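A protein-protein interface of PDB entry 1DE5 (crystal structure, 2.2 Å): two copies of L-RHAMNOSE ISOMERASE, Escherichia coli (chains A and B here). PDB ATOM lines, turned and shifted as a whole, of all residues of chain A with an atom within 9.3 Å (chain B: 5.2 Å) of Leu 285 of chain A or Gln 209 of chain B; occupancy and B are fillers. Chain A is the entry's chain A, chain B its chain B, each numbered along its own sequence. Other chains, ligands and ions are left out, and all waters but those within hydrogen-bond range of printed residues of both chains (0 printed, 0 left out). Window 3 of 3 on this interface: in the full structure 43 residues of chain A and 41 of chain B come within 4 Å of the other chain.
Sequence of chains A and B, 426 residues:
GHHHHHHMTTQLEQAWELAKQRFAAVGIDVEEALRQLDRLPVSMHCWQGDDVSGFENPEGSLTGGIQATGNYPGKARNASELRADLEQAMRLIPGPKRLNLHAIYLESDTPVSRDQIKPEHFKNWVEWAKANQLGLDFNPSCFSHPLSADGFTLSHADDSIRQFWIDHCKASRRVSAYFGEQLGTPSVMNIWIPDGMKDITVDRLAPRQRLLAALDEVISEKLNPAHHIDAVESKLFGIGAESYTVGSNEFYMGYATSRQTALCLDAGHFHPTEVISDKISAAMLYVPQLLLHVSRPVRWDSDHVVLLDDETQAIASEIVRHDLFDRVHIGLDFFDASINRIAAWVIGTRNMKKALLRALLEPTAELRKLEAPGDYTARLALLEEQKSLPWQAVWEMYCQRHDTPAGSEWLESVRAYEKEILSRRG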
ATOM      1  N   MET A 253      27.646   6.343 -13.766  1.00  0.00           N
ATOM      2  CA  MET A 253      26.331   5.818 -14.012  1.00  0.00           C
ATOM      3  C   MET A 253      25.990   5.067 -12.717  1.00  0.00           C
ATOM      4  O   MET A 253      24.960   5.259 -12.058  1.00  0.00           O
ATOM      5  CB  MET A 253      26.245   4.848 -15.221  1.00  0.00           C
ATOM      6  CG  MET A 253      24.828   4.228 -15.319  1.00  0.00           C
ATOM      7  SD  MET A 253      23.718   5.451 -16.035  1.00  0.00           S
ATOM      8  CE  MET A 253      22.098   4.679 -15.799  1.00  0.00           C
ATOM      9  N   THR A 257      22.964   6.408 -10.123  1.00  0.00           N
ATOM     10  CA  THR A 257      21.840   5.497  -9.966  1.00  0.00           C
ATOM     11  C   THR A 257      21.618   5.144  -8.523  1.00  0.00           C
ATOM     12  O   THR A 257      20.486   5.207  -8.038  1.00  0.00           O
ATOM     13  CB  THR A 257      22.039   4.154 -10.746  1.00  0.00           C
ATOM     14  OG1 THR A 257      22.045   4.342 -12.156  1.00  0.00           O
ATOM     15  CG2 THR A 257      20.923   3.188 -10.397  1.00  0.00           C
ATOM     16  N   GLN A 260      20.946   8.512  -6.768  1.00  0.00           N
ATOM     17  CA  GLN A 260      19.910   9.378  -7.328  1.00  0.00           C
ATOM     18  C   GLN A 260      20.296  10.844  -7.489  1.00  0.00           C
ATOM     19  O   GLN A 260      19.550  11.822  -7.238  1.00  0.00           O
ATOM     20  CB  GLN A 260      18.581   9.175  -6.670  1.00  0.00           C
ATOM     21  CG  GLN A 260      18.299   7.687  -6.771  1.00  0.00           C
ATOM     22  CD  GLN A 260      17.657   7.528  -8.117  1.00  0.00           C
ATOM     23  OE1 GLN A 260      16.626   8.156  -8.346  1.00  0.00           O
ATOM     24  NE2 GLN A 260      18.303   6.788  -9.011  1.00  0.00           N
ATOM     25  N   LEU A 263      22.850  12.842 -13.665  1.00  0.00           N
ATOM     26  CA  LEU A 263      23.983  12.335 -14.377  1.00  0.00           C
ATOM     27  C   LEU A 263      24.320  13.296 -15.487  1.00  0.00           C
ATOM     28  O   LEU A 263      23.431  13.715 -16.226  1.00  0.00           O
ATOM     29  CB  LEU A 263      23.720  10.918 -14.922  1.00  0.00           C
ATOM     30  CG  LEU A 263      24.857  10.480 -15.848  1.00  0.00           C
ATOM     31  CD1 LEU A 263      26.073  10.161 -14.983  1.00  0.00           C
ATOM     32  CD2 LEU A 263      24.452   9.198 -16.559  1.00  0.00           C
ATOM     33  N   LYS A 279      22.368   7.700 -25.026  1.00  0.00           N
ATOM     34  CA  LYS A 279      22.365   7.492 -23.574  1.00  0.00           C
ATOM     35  C   LYS A 279      21.205   8.022 -22.813  1.00  0.00           C
ATOM     36  O   LYS A 279      20.812   7.378 -21.833  1.00  0.00           O
ATOM     37  CB  LYS A 279      23.683   7.798 -22.931  1.00  0.00           C
ATOM     38  CG  LYS A 279      24.837   7.309 -23.812  1.00  0.00           C
ATOM     39  CD  LYS A 279      26.204   7.763 -23.357  1.00  0.00           C
ATOM     40  CE  LYS A 279      27.361   7.116 -24.114  1.00  0.00           C
ATOM     41  NZ  LYS A 279      27.471   5.680 -23.878  1.00  0.00           N
ATOM     42  N   ILE A 280      20.657   9.138 -23.318  1.00  0.00           N
ATOM     43  CA  ILE A 280      19.489   9.793 -22.713  1.00  0.00           C
ATOM     44  C   ILE A 280      18.301   8.845 -22.302  1.00  0.00           C
ATOM     45  O   ILE A 280      17.872   8.779 -21.150  1.00  0.00           O
ATOM     46  CB  ILE A 280      18.996  10.888 -23.679  1.00  0.00           C
ATOM     47  CG1 ILE A 280      20.089  11.941 -23.913  1.00  0.00           C
ATOM     48  CG2 ILE A 280      17.686  11.507 -23.155  1.00  0.00           C
ATOM     49  CD1 ILE A 280      19.876  12.905 -25.111  1.00  0.00           C
ATOM     50  N   SER A 281      17.731   8.084 -23.247  1.00  0.00           N
ATOM     51  CA  SER A 281      16.583   7.213 -22.939  1.00  0.00           C
ATOM     52  C   SER A 281      16.968   6.133 -21.962  1.00  0.00           C
ATOM     53  O   SER A 281      16.146   5.744 -21.139  1.00  0.00           O
ATOM     54  CB  SER A 281      16.002   6.554 -24.209  1.00  0.00           C
ATOM     55  OG  SER A 281      17.049   5.934 -24.968  1.00  0.00           O
ATOM     56  N   ALA A 282      18.226   5.647 -22.102  1.00  0.00           N
ATOM     57  CA  ALA A 282      18.761   4.632 -21.203  1.00  0.00           C
ATOM     58  C   ALA A 282      18.899   5.188 -19.775  1.00  0.00           C
ATOM     59  O   ALA A 282      18.362   4.697 -18.773  1.00  0.00           O
ATOM     60  CB  ALA A 282      20.138   4.132 -21.694  1.00  0.00           C
ATOM     61  N   ALA A 283      19.687   6.244 -19.709  1.00  0.00           N
ATOM     62  CA  ALA A 283      20.019   6.893 -18.441  1.00  0.00           C
ATOM     63  C   ALA A 283      18.806   7.254 -17.562  1.00  0.00           C
ATOM     64  O   ALA A 283      18.697   6.914 -16.397  1.00  0.00           O
ATOM     65  CB  ALA A 283      20.972   8.065 -18.750  1.00  0.00           C
ATOM     66  N   MET A 284      17.878   7.949 -18.186  1.00  0.00           N
ATOM     67  CA  MET A 284      16.662   8.422 -17.558  1.00  0.00           C
ATOM     68  C   MET A 284      15.764   7.373 -16.874  1.00  0.00           C
ATOM     69  O   MET A 284      14.918   7.762 -16.040  1.00  0.00           O
ATOM     70  CB  MET A 284      15.904   9.250 -18.601  1.00  0.00           C
ATOM     71  CG  MET A 284      15.179   8.341 -19.572  1.00  0.00           C
ATOM     72  SD  MET A 284      14.202   9.271 -20.790  1.00  0.00           S
ATOM     73  CE  MET A 284      12.704   9.554 -19.784  1.00  0.00           C
ATOM     74  N   LEU A 285      15.933   6.054 -17.209  1.00  0.00           N
ATOM     75  CA  LEU A 285      15.117   5.019 -16.577  1.00  0.00           C
ATOM     76  C   LEU A 285      15.655   4.682 -15.247  1.00  0.00           C
ATOM     77  O   LEU A 285      15.029   3.916 -14.564  1.00  0.00           O
ATOM     78  CB  LEU A 285      15.116   3.672 -17.298  1.00  0.00           C
ATOM     79  CG  LEU A 285      14.303   3.709 -18.591  1.00  0.00           C
ATOM     80  CD1 LEU A 285      14.585   2.465 -19.449  1.00  0.00           C
ATOM     81  CD2 LEU A 285      12.824   3.821 -18.241  1.00  0.00           C
ATOM     82  N   TYR A 286      16.830   5.238 -14.911  1.00  0.00           N
ATOM     83  CA  TYR A 286      17.507   4.966 -13.638  1.00  0.00           C
ATOM     84  C   TYR A 286      17.914   6.191 -12.832  1.00  0.00           C
ATOM     85  O   TYR A 286      18.114   6.119 -11.631  1.00  0.00           O
ATOM     86  CB  TYR A 286      18.757   4.098 -13.836  1.00  0.00           C
ATOM     87  CG  TYR A 286      18.424   2.828 -14.559  1.00  0.00           C
ATOM     88  CD1 TYR A 286      18.634   2.749 -15.934  1.00  0.00           C
ATOM     89  CD2 TYR A 286      17.923   1.712 -13.880  1.00  0.00           C
ATOM     90  CE1 TYR A 286      18.356   1.566 -16.608  1.00  0.00           C
ATOM     91  CE2 TYR A 286      17.637   0.515 -14.538  1.00  0.00           C
ATOM     92  CZ  TYR A 286      17.844   0.470 -15.915  1.00  0.00           C
ATOM     93  OH  TYR A 286      17.532  -0.639 -16.636  1.00  0.00           O
ATOM     94  N   VAL A 287      18.089   7.306 -13.497  1.00  0.00           N
ATOM     95  CA  VAL A 287      18.499   8.495 -12.795  1.00  0.00           C
ATOM     96  C   VAL A 287      17.456   9.529 -13.001  1.00  0.00           C
ATOM     97  O   VAL A 287      16.818   9.611 -14.042  1.00  0.00           O
ATOM     98  CB  VAL A 287      19.882   9.018 -13.204  1.00  0.00           C
ATOM     99  CG1 VAL A 287      21.058   8.053 -12.926  1.00  0.00           C
ATOM    100  CG2 VAL A 287      19.876   9.658 -14.571  1.00  0.00           C
ATOM    101  N   PRO A 288      17.302  10.330 -11.969  1.00  0.00           N
ATOM    102  CA  PRO A 288      16.264  11.316 -11.909  1.00  0.00           C
ATOM    103  C   PRO A 288      16.351  12.360 -12.945  1.00  0.00           C
ATOM    104  O   PRO A 288      15.347  12.789 -13.506  1.00  0.00           O
ATOM    105  CB  PRO A 288      16.403  11.951 -10.516  1.00  0.00           C
ATOM    106  CG  PRO A 288      17.840  11.686 -10.068  1.00  0.00           C
ATOM    107  CD  PRO A 288      18.228  10.442 -10.814  1.00  0.00           C
ATOM    108  N   GLN A 289      17.554  12.801 -13.159  1.00  0.00           N
ATOM    109  CA  GLN A 289      17.711  13.856 -14.101  1.00  0.00           C
ATOM    110  C   GLN A 289      18.986  13.719 -14.838  1.00  0.00           C
ATOM    111  O   GLN A 289      19.877  13.040 -14.348  1.00  0.00           O
ATOM    112  CB  GLN A 289      17.864  15.171 -13.337  1.00  0.00           C
ATOM    113  CG  GLN A 289      16.672  16.094 -13.514  1.00  0.00           C
ATOM    114  CD  GLN A 289      16.293  16.542 -12.144  1.00  0.00           C
ATOM    115  OE1 GLN A 289      16.750  15.906 -11.164  1.00  0.00           O
ATOM    116  NE2 GLN A 289      15.503  17.614 -12.085  1.00  0.00           N
ATOM    117  N   LEU A 290      19.044  14.502 -15.913  1.00  0.00           N
ATOM    118  CA  LEU A 290      20.165  14.589 -16.800  1.00  0.00           C
ATOM    119  C   LEU A 290      20.571  15.990 -17.061  1.00  0.00           C
ATOM    120  O   LEU A 290      19.756  16.887 -17.221  1.00  0.00           O
ATOM    121  CB  LEU A 290      19.851  14.064 -18.232  1.00  0.00           C
ATOM    122  CG  LEU A 290      19.481  12.580 -18.297  1.00  0.00           C
ATOM    123  CD1 LEU A 290      19.127  12.215 -19.737  1.00  0.00           C
ATOM    124  CD2 LEU A 290      20.646  11.745 -17.763  1.00  0.00           C
ATOM    125  N   HIS A 322      10.855  12.653 -26.247  1.00  0.00           N
ATOM    126  CA  HIS A 322      10.202  12.192 -25.038  1.00  0.00           C
ATOM    127  C   HIS A 322       9.715  13.316 -24.091  1.00  0.00           C
ATOM    128  O   HIS A 322       9.601  13.142 -22.881  1.00  0.00           O
ATOM    129  CB  HIS A 322      11.063  11.120 -24.412  1.00  0.00           C
ATOM    130  CG  HIS A 322      11.603  10.180 -25.496  1.00  0.00           C
ATOM    131  ND1 HIS A 322      10.773   9.315 -26.203  1.00  0.00           N
ATOM    132  CD2 HIS A 322      12.894   9.951 -25.928  1.00  0.00           C
ATOM    133  CE1 HIS A 322      11.554   8.599 -27.003  1.00  0.00           C
ATOM    134  NE2 HIS A 322      12.837   8.936 -26.860  1.00  0.00           N
ATOM    135  N   LEU A 324      11.016  15.627 -22.824  1.00  0.00           N
ATOM    136  CA  LEU A 324      11.837  15.755 -21.659  1.00  0.00           C
ATOM    137  C   LEU A 324      12.053  17.208 -21.244  1.00  0.00           C
ATOM    138  O   LEU A 324      13.180  17.656 -21.114  1.00  0.00           O
ATOM    139  CB  LEU A 324      13.175  15.098 -22.010  1.00  0.00           C
ATOM    140  CG  LEU A 324      13.226  13.648 -21.522  1.00  0.00           C
ATOM    141  CD1 LEU A 324      11.809  13.214 -21.194  1.00  0.00           C
ATOM    142  CD2 LEU A 324      13.918  12.723 -22.535  1.00  0.00           C
ATOM    143  N   ARG A 327      13.206  16.992 -16.855  1.00  0.00           N
ATOM    144  CA  ARG A 327      14.293  16.222 -16.331  1.00  0.00           C
ATOM    145  C   ARG A 327      15.604  16.399 -17.103  1.00  0.00           C
ATOM    146  O   ARG A 327      16.669  15.959 -16.666  1.00  0.00           O
ATOM    147  CB  ARG A 327      13.895  14.789 -16.381  1.00  0.00           C
ATOM    148  CG  ARG A 327      12.577  14.599 -15.695  1.00  0.00           C
ATOM    149  CD  ARG A 327      12.635  13.300 -14.934  1.00  0.00           C
ATOM    150  NE  ARG A 327      12.267  12.193 -15.789  1.00  0.00           N
ATOM    151  CZ  ARG A 327      12.877  11.005 -15.847  1.00  0.00           C
ATOM    152  NH1 ARG A 327      13.963  10.669 -15.123  1.00  0.00           N
ATOM    153  NH2 ARG A 327      12.354  10.101 -16.675  1.00  0.00           N
ATOM    154  N   ARG A 368       6.611   7.441 -35.128  1.00  0.00           N
ATOM    155  CA  ARG A 368       6.611   6.485 -34.049  1.00  0.00           C
ATOM    156  C   ARG A 368       5.675   5.332 -34.329  1.00  0.00           C
ATOM    157  O   ARG A 368       5.887   4.133 -34.030  1.00  0.00           O
ATOM    158  CB  ARG A 368       5.967   7.298 -32.943  1.00  0.00           C
ATOM    159  CG  ARG A 368       6.352   6.938 -31.529  1.00  0.00           C
ATOM    160  CD  ARG A 368       5.524   7.804 -30.573  1.00  0.00           C
ATOM    161  NE  ARG A 368       6.247   8.389 -29.444  1.00  0.00           N
ATOM    162  CZ  ARG A 368       7.577   8.552 -29.303  1.00  0.00           C
ATOM    163  NH1 ARG A 368       8.474   8.193 -30.229  1.00  0.00           N
ATOM    164  NH2 ARG A 368       8.040   9.104 -28.174  1.00  0.00           N
ATOM    165  N   LEU B 205      13.220   4.897 -26.321  1.00  0.00           N
ATOM    166  CA  LEU B 205      12.641   4.883 -24.963  1.00  0.00           C
ATOM    167  C   LEU B 205      11.634   3.768 -24.658  1.00  0.00           C
ATOM    168  O   LEU B 205      11.769   3.055 -23.683  1.00  0.00           O
ATOM    169  CB  LEU B 205      12.011   6.241 -24.536  1.00  0.00           C
ATOM    170  CG  LEU B 205      11.457   6.181 -23.107  1.00  0.00           C
ATOM    171  CD1 LEU B 205      12.591   5.899 -22.144  1.00  0.00           C
ATOM    172  CD2 LEU B 205      10.771   7.486 -22.717  1.00  0.00           C
ATOM    173  N   ALA B 206      10.572   3.625 -25.442  1.00  0.00           N
ATOM    174  CA  ALA B 206       9.514   2.579 -25.186  1.00  0.00           C
ATOM    175  C   ALA B 206      10.019   1.135 -25.024  1.00  0.00           C
ATOM    176  O   ALA B 206       9.633   0.419 -24.088  1.00  0.00           O
ATOM    177  CB  ALA B 206       8.268   2.707 -26.080  1.00  0.00           C
ATOM    178  N   PRO B 207      10.935   0.721 -25.919  1.00  0.00           N
ATOM    179  CA  PRO B 207      11.535  -0.581 -25.810  1.00  0.00           C
ATOM    180  C   PRO B 207      12.272  -0.786 -24.496  1.00  0.00           C
ATOM    181  O   PRO B 207      12.101  -1.817 -23.827  1.00  0.00           O
ATOM    182  CB  PRO B 207      12.475  -0.705 -26.983  1.00  0.00           C
ATOM    183  CG  PRO B 207      11.949   0.284 -28.008  1.00  0.00           C
ATOM    184  CD  PRO B 207      11.304   1.381 -27.189  1.00  0.00           C
ATOM    185  N   ARG B 208      13.068   0.227 -24.116  1.00  0.00           N
ATOM    186  CA  ARG B 208      13.860   0.197 -22.873  1.00  0.00           C
ATOM    187  C   ARG B 208      12.930   0.102 -21.671  1.00  0.00           C
ATOM    188  O   ARG B 208      13.195  -0.653 -20.719  1.00  0.00           O
ATOM    189  CB  ARG B 208      14.881   1.358 -22.757  1.00  0.00           C
ATOM    190  CG  ARG B 208      15.815   1.543 -23.960  1.00  0.00           C
ATOM    191  CD  ARG B 208      16.968   2.554 -23.804  1.00  0.00           C
ATOM    192  NE  ARG B 208      18.070   2.093 -24.651  1.00  0.00           N
ATOM    193  CZ  ARG B 208      18.917   2.878 -25.277  1.00  0.00           C
ATOM    194  NH1 ARG B 208      18.904   4.210 -25.192  1.00  0.00           N
ATOM    195  NH2 ARG B 208      19.802   2.302 -26.036  1.00  0.00           N
ATOM    196  N   GLN B 209      11.811   0.857 -21.727  1.00  0.00           N
ATOM    197  CA  GLN B 209      10.811   0.808 -20.644  1.00  0.00           C
ATOM    198  C   GLN B 209      10.216  -0.596 -20.492  1.00  0.00           C
ATOM    199  O   GLN B 209      10.061  -1.106 -19.383  1.00  0.00           O
ATOM    200  CB  GLN B 209       9.704   1.808 -20.877  1.00  0.00           C
ATOM    201  CG  GLN B 209      10.164   3.195 -20.463  1.00  0.00           C
ATOM    202  CD  GLN B 209       9.141   4.158 -20.978  1.00  0.00           C
ATOM    203  OE1 GLN B 209       8.554   3.893 -22.048  1.00  0.00           O
ATOM    204  NE2 GLN B 209       8.903   5.224 -20.203  1.00  0.00           N
ATOM    205  N   ARG B 210       9.952  -1.228 -21.624  1.00  0.00           N
ATOM    206  CA  ARG B 210       9.439  -2.591 -21.611  1.00  0.00           C
ATOM    207  C   ARG B 210      10.518  -3.575 -21.205  1.00  0.00           C
ATOM    208  O   ARG B 210      10.303  -4.666 -20.686  1.00  0.00           O
ATOM    209  CB  ARG B 210       9.142  -3.034 -23.014  1.00  0.00           C
ATOM    210  CG  ARG B 210       7.959  -2.413 -23.651  1.00  0.00           C
ATOM    211  CD  ARG B 210       7.991  -2.939 -25.079  1.00  0.00           C
ATOM    212  NE  ARG B 210       7.431  -1.914 -25.898  1.00  0.00           N
ATOM    213  CZ  ARG B 210       7.883  -1.440 -27.007  1.00  0.00           C
ATOM    214  NH1 ARG B 210       8.982  -1.868 -27.624  1.00  0.00           N
ATOM    215  NH2 ARG B 210       7.180  -0.451 -27.505  1.00  0.00           N
ATOM    216  N   LEU B 211      11.735  -3.239 -21.522  1.00  0.00           N
ATOM    217  CA  LEU B 211      12.784  -4.154 -21.144  1.00  0.00           C
ATOM    218  C   LEU B 211      12.908  -4.082 -19.637  1.00  0.00           C
ATOM    219  O   LEU B 211      12.964  -5.055 -18.898  1.00  0.00           O
ATOM    220  CB  LEU B 211      14.103  -3.742 -21.845  1.00  0.00           C
ATOM    221  CG  LEU B 211      15.271  -4.641 -21.437  1.00  0.00           C
ATOM    222  CD1 LEU B 211      14.887  -6.109 -21.633  1.00  0.00           C
ATOM    223  CD2 LEU B 211      16.439  -4.305 -22.330  1.00  0.00           C
ATOM    224  N   LEU B 212      12.932  -2.868 -19.144  1.00  0.00           N
ATOM    225  CA  LEU B 212      13.007  -2.712 -17.702  1.00  0.00           C
ATOM    226  C   LEU B 212      11.903  -3.524 -16.975  1.00  0.00           C
ATOM    227  O   LEU B 212      12.114  -4.296 -15.987  1.00  0.00           O
ATOM    228  CB  LEU B 212      12.706  -1.227 -17.494  1.00  0.00           C
ATOM    229  CG  LEU B 212      12.958  -0.765 -16.066  1.00  0.00           C
ATOM    230  CD1 LEU B 212      13.678  -1.854 -15.269  1.00  0.00           C
ATOM    231  CD2 LEU B 212      13.779   0.529 -16.088  1.00  0.00           C
ATOM    232  N   ALA B 213      10.656  -3.325 -17.441  1.00  0.00           N
ATOM    233  CA  ALA B 213       9.536  -4.020 -16.787  1.00  0.00           C
ATOM    234  C   ALA B 213       9.610  -5.559 -16.808  1.00  0.00           C
ATOM    235  O   ALA B 213       9.399  -6.231 -15.829  1.00  0.00           O
ATOM    236  CB  ALA B 213       8.204  -3.442 -17.233  1.00  0.00           C
ATOM    237  N   ALA B 214      10.018  -6.084 -17.958  1.00  0.00           N
ATOM    238  CA  ALA B 214      10.155  -7.499 -18.215  1.00  0.00           C
ATOM    239  C   ALA B 214      11.181  -8.178 -17.325  1.00  0.00           C
ATOM    240  O   ALA B 214      10.939  -9.297 -16.790  1.00  0.00           O
ATOM    241  CB  ALA B 214      10.606  -7.544 -19.664  1.00  0.00           C
ATOM    242  N   PHE B 251      21.975   1.311 -19.867  1.00  0.00           N
ATOM    243  CA  PHE B 251      20.752   0.558 -19.467  1.00  0.00           C
ATOM    244  C   PHE B 251      21.049  -0.517 -18.388  1.00  0.00           C
ATOM    245  O   PHE B 251      20.484  -0.609 -17.301  1.00  0.00           O
ATOM    246  CB  PHE B 251      20.083  -0.112 -20.755  1.00  0.00           C
ATOM    247  CG  PHE B 251      18.792  -0.776 -20.346  1.00  0.00           C
ATOM    248  CD1 PHE B 251      17.584  -0.075 -20.314  1.00  0.00           C
ATOM    249  CD2 PHE B 251      18.825  -2.053 -19.792  1.00  0.00           C
ATOM    250  CE1 PHE B 251      16.430  -0.675 -19.822  1.00  0.00           C
ATOM    251  CE2 PHE B 251      17.686  -2.671 -19.282  1.00  0.00           C
ATOM    252  CZ  PHE B 251      16.481  -1.976 -19.321  1.00  0.00           C
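Of the printed residues of chain B, Ala 282 of chain A touches Arg 208 (3.5 Å) and Phe 251 (3.8 Å).
Leu 285 of chain A touches just these residues of chain B: Arg 208, Gln 209, Leu 212 and Phe 251.
Printed residues of chain B within 4 Å of Tyr 286 of chain A: Leu 212 and Phe 251.
Arg 368 of chain A touches none of the printed residues of chain B.
Of the printed residues of chain A, Leu 205 of chain B touches Ser 281 (3.7 Å), Met 284 (3.97 Å) and His 322 (3.4 Å).
No residue of chain A comes within 4 Å of Ala 206 of chain B.
Ala 213 of chain B touches none of the printed residues of chain A.
The nearest residue of chain B that does not touch Leu 285 of chain A is Leu 205 of chain B (4.4 Å).
OH of Tyr 286 of chain A sits at hydrogen-bond distance from O of Phe 251 of chain B, at 3.0 Å.
N of Ala 282 of chain A lies close to NH1 of Arg 208 of chain B, 3.5 Å away.
OG of Ser 281 of chain A sits at hydrogen-bond distance from NH1 of Arg 208 of chain B, at 2.5 Å.
NE2 of Gln 260 of chain A is in hydrogen-bond range of O of Tyr 286 of chain A (2.7 Å).
NH2 of Arg 368 of chain A sits at hydrogen-bond distance from ND1 of His 322 of chain A (3.4 Å).
The guanidinium group (NH1) of Arg 327 of chain A lies within hydrogen-bond range of the backbone carbonyl oxygen (O) of Met 284 of chain A (3.2 Å).
Printed residues of chain A that touch a printed residue of chain B: Ser 281, Ala 282, Met 284, Leu 285, Tyr 286 and His 322.
Along chain A the printed residues that touch a printed residue of chain B span positions 281 to 322.
Among the printed residues, no Asp or Glu carboxylate lies within 4 Å of a Lys or Arg side-chain nitrogen of the other chain.
No position is printed for both chains.
Of the 12 pairs that touch across the chains among the printed residues, none has its exchanged pair printed and touching as well.
Among the printed residues, merely in contact across the chains: Ser 281 of chain A with Leu 205 of chain B (3.7 Å), Ala 282 of chain A with Phe 251 of chain B (3.8 Å), Met 284 of chain A with Leu 205 of chain B (3.97 Å), Leu 285 of chain A with Arg 208 of chain B (3.5 Å), Leu 285 of chain A with Gln 209 of chain B (3.5 Å), Leu 285 of chain A with Leu 212 of chain B (3.6 Å), Leu 285 of chain A with Phe 251 of chain B (3.7 Å), Tyr 286 of chain A with Leu 212 of chain B (3.97 Å) and His 322 of chain A with Leu 205 of chain B (3.4 Å).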
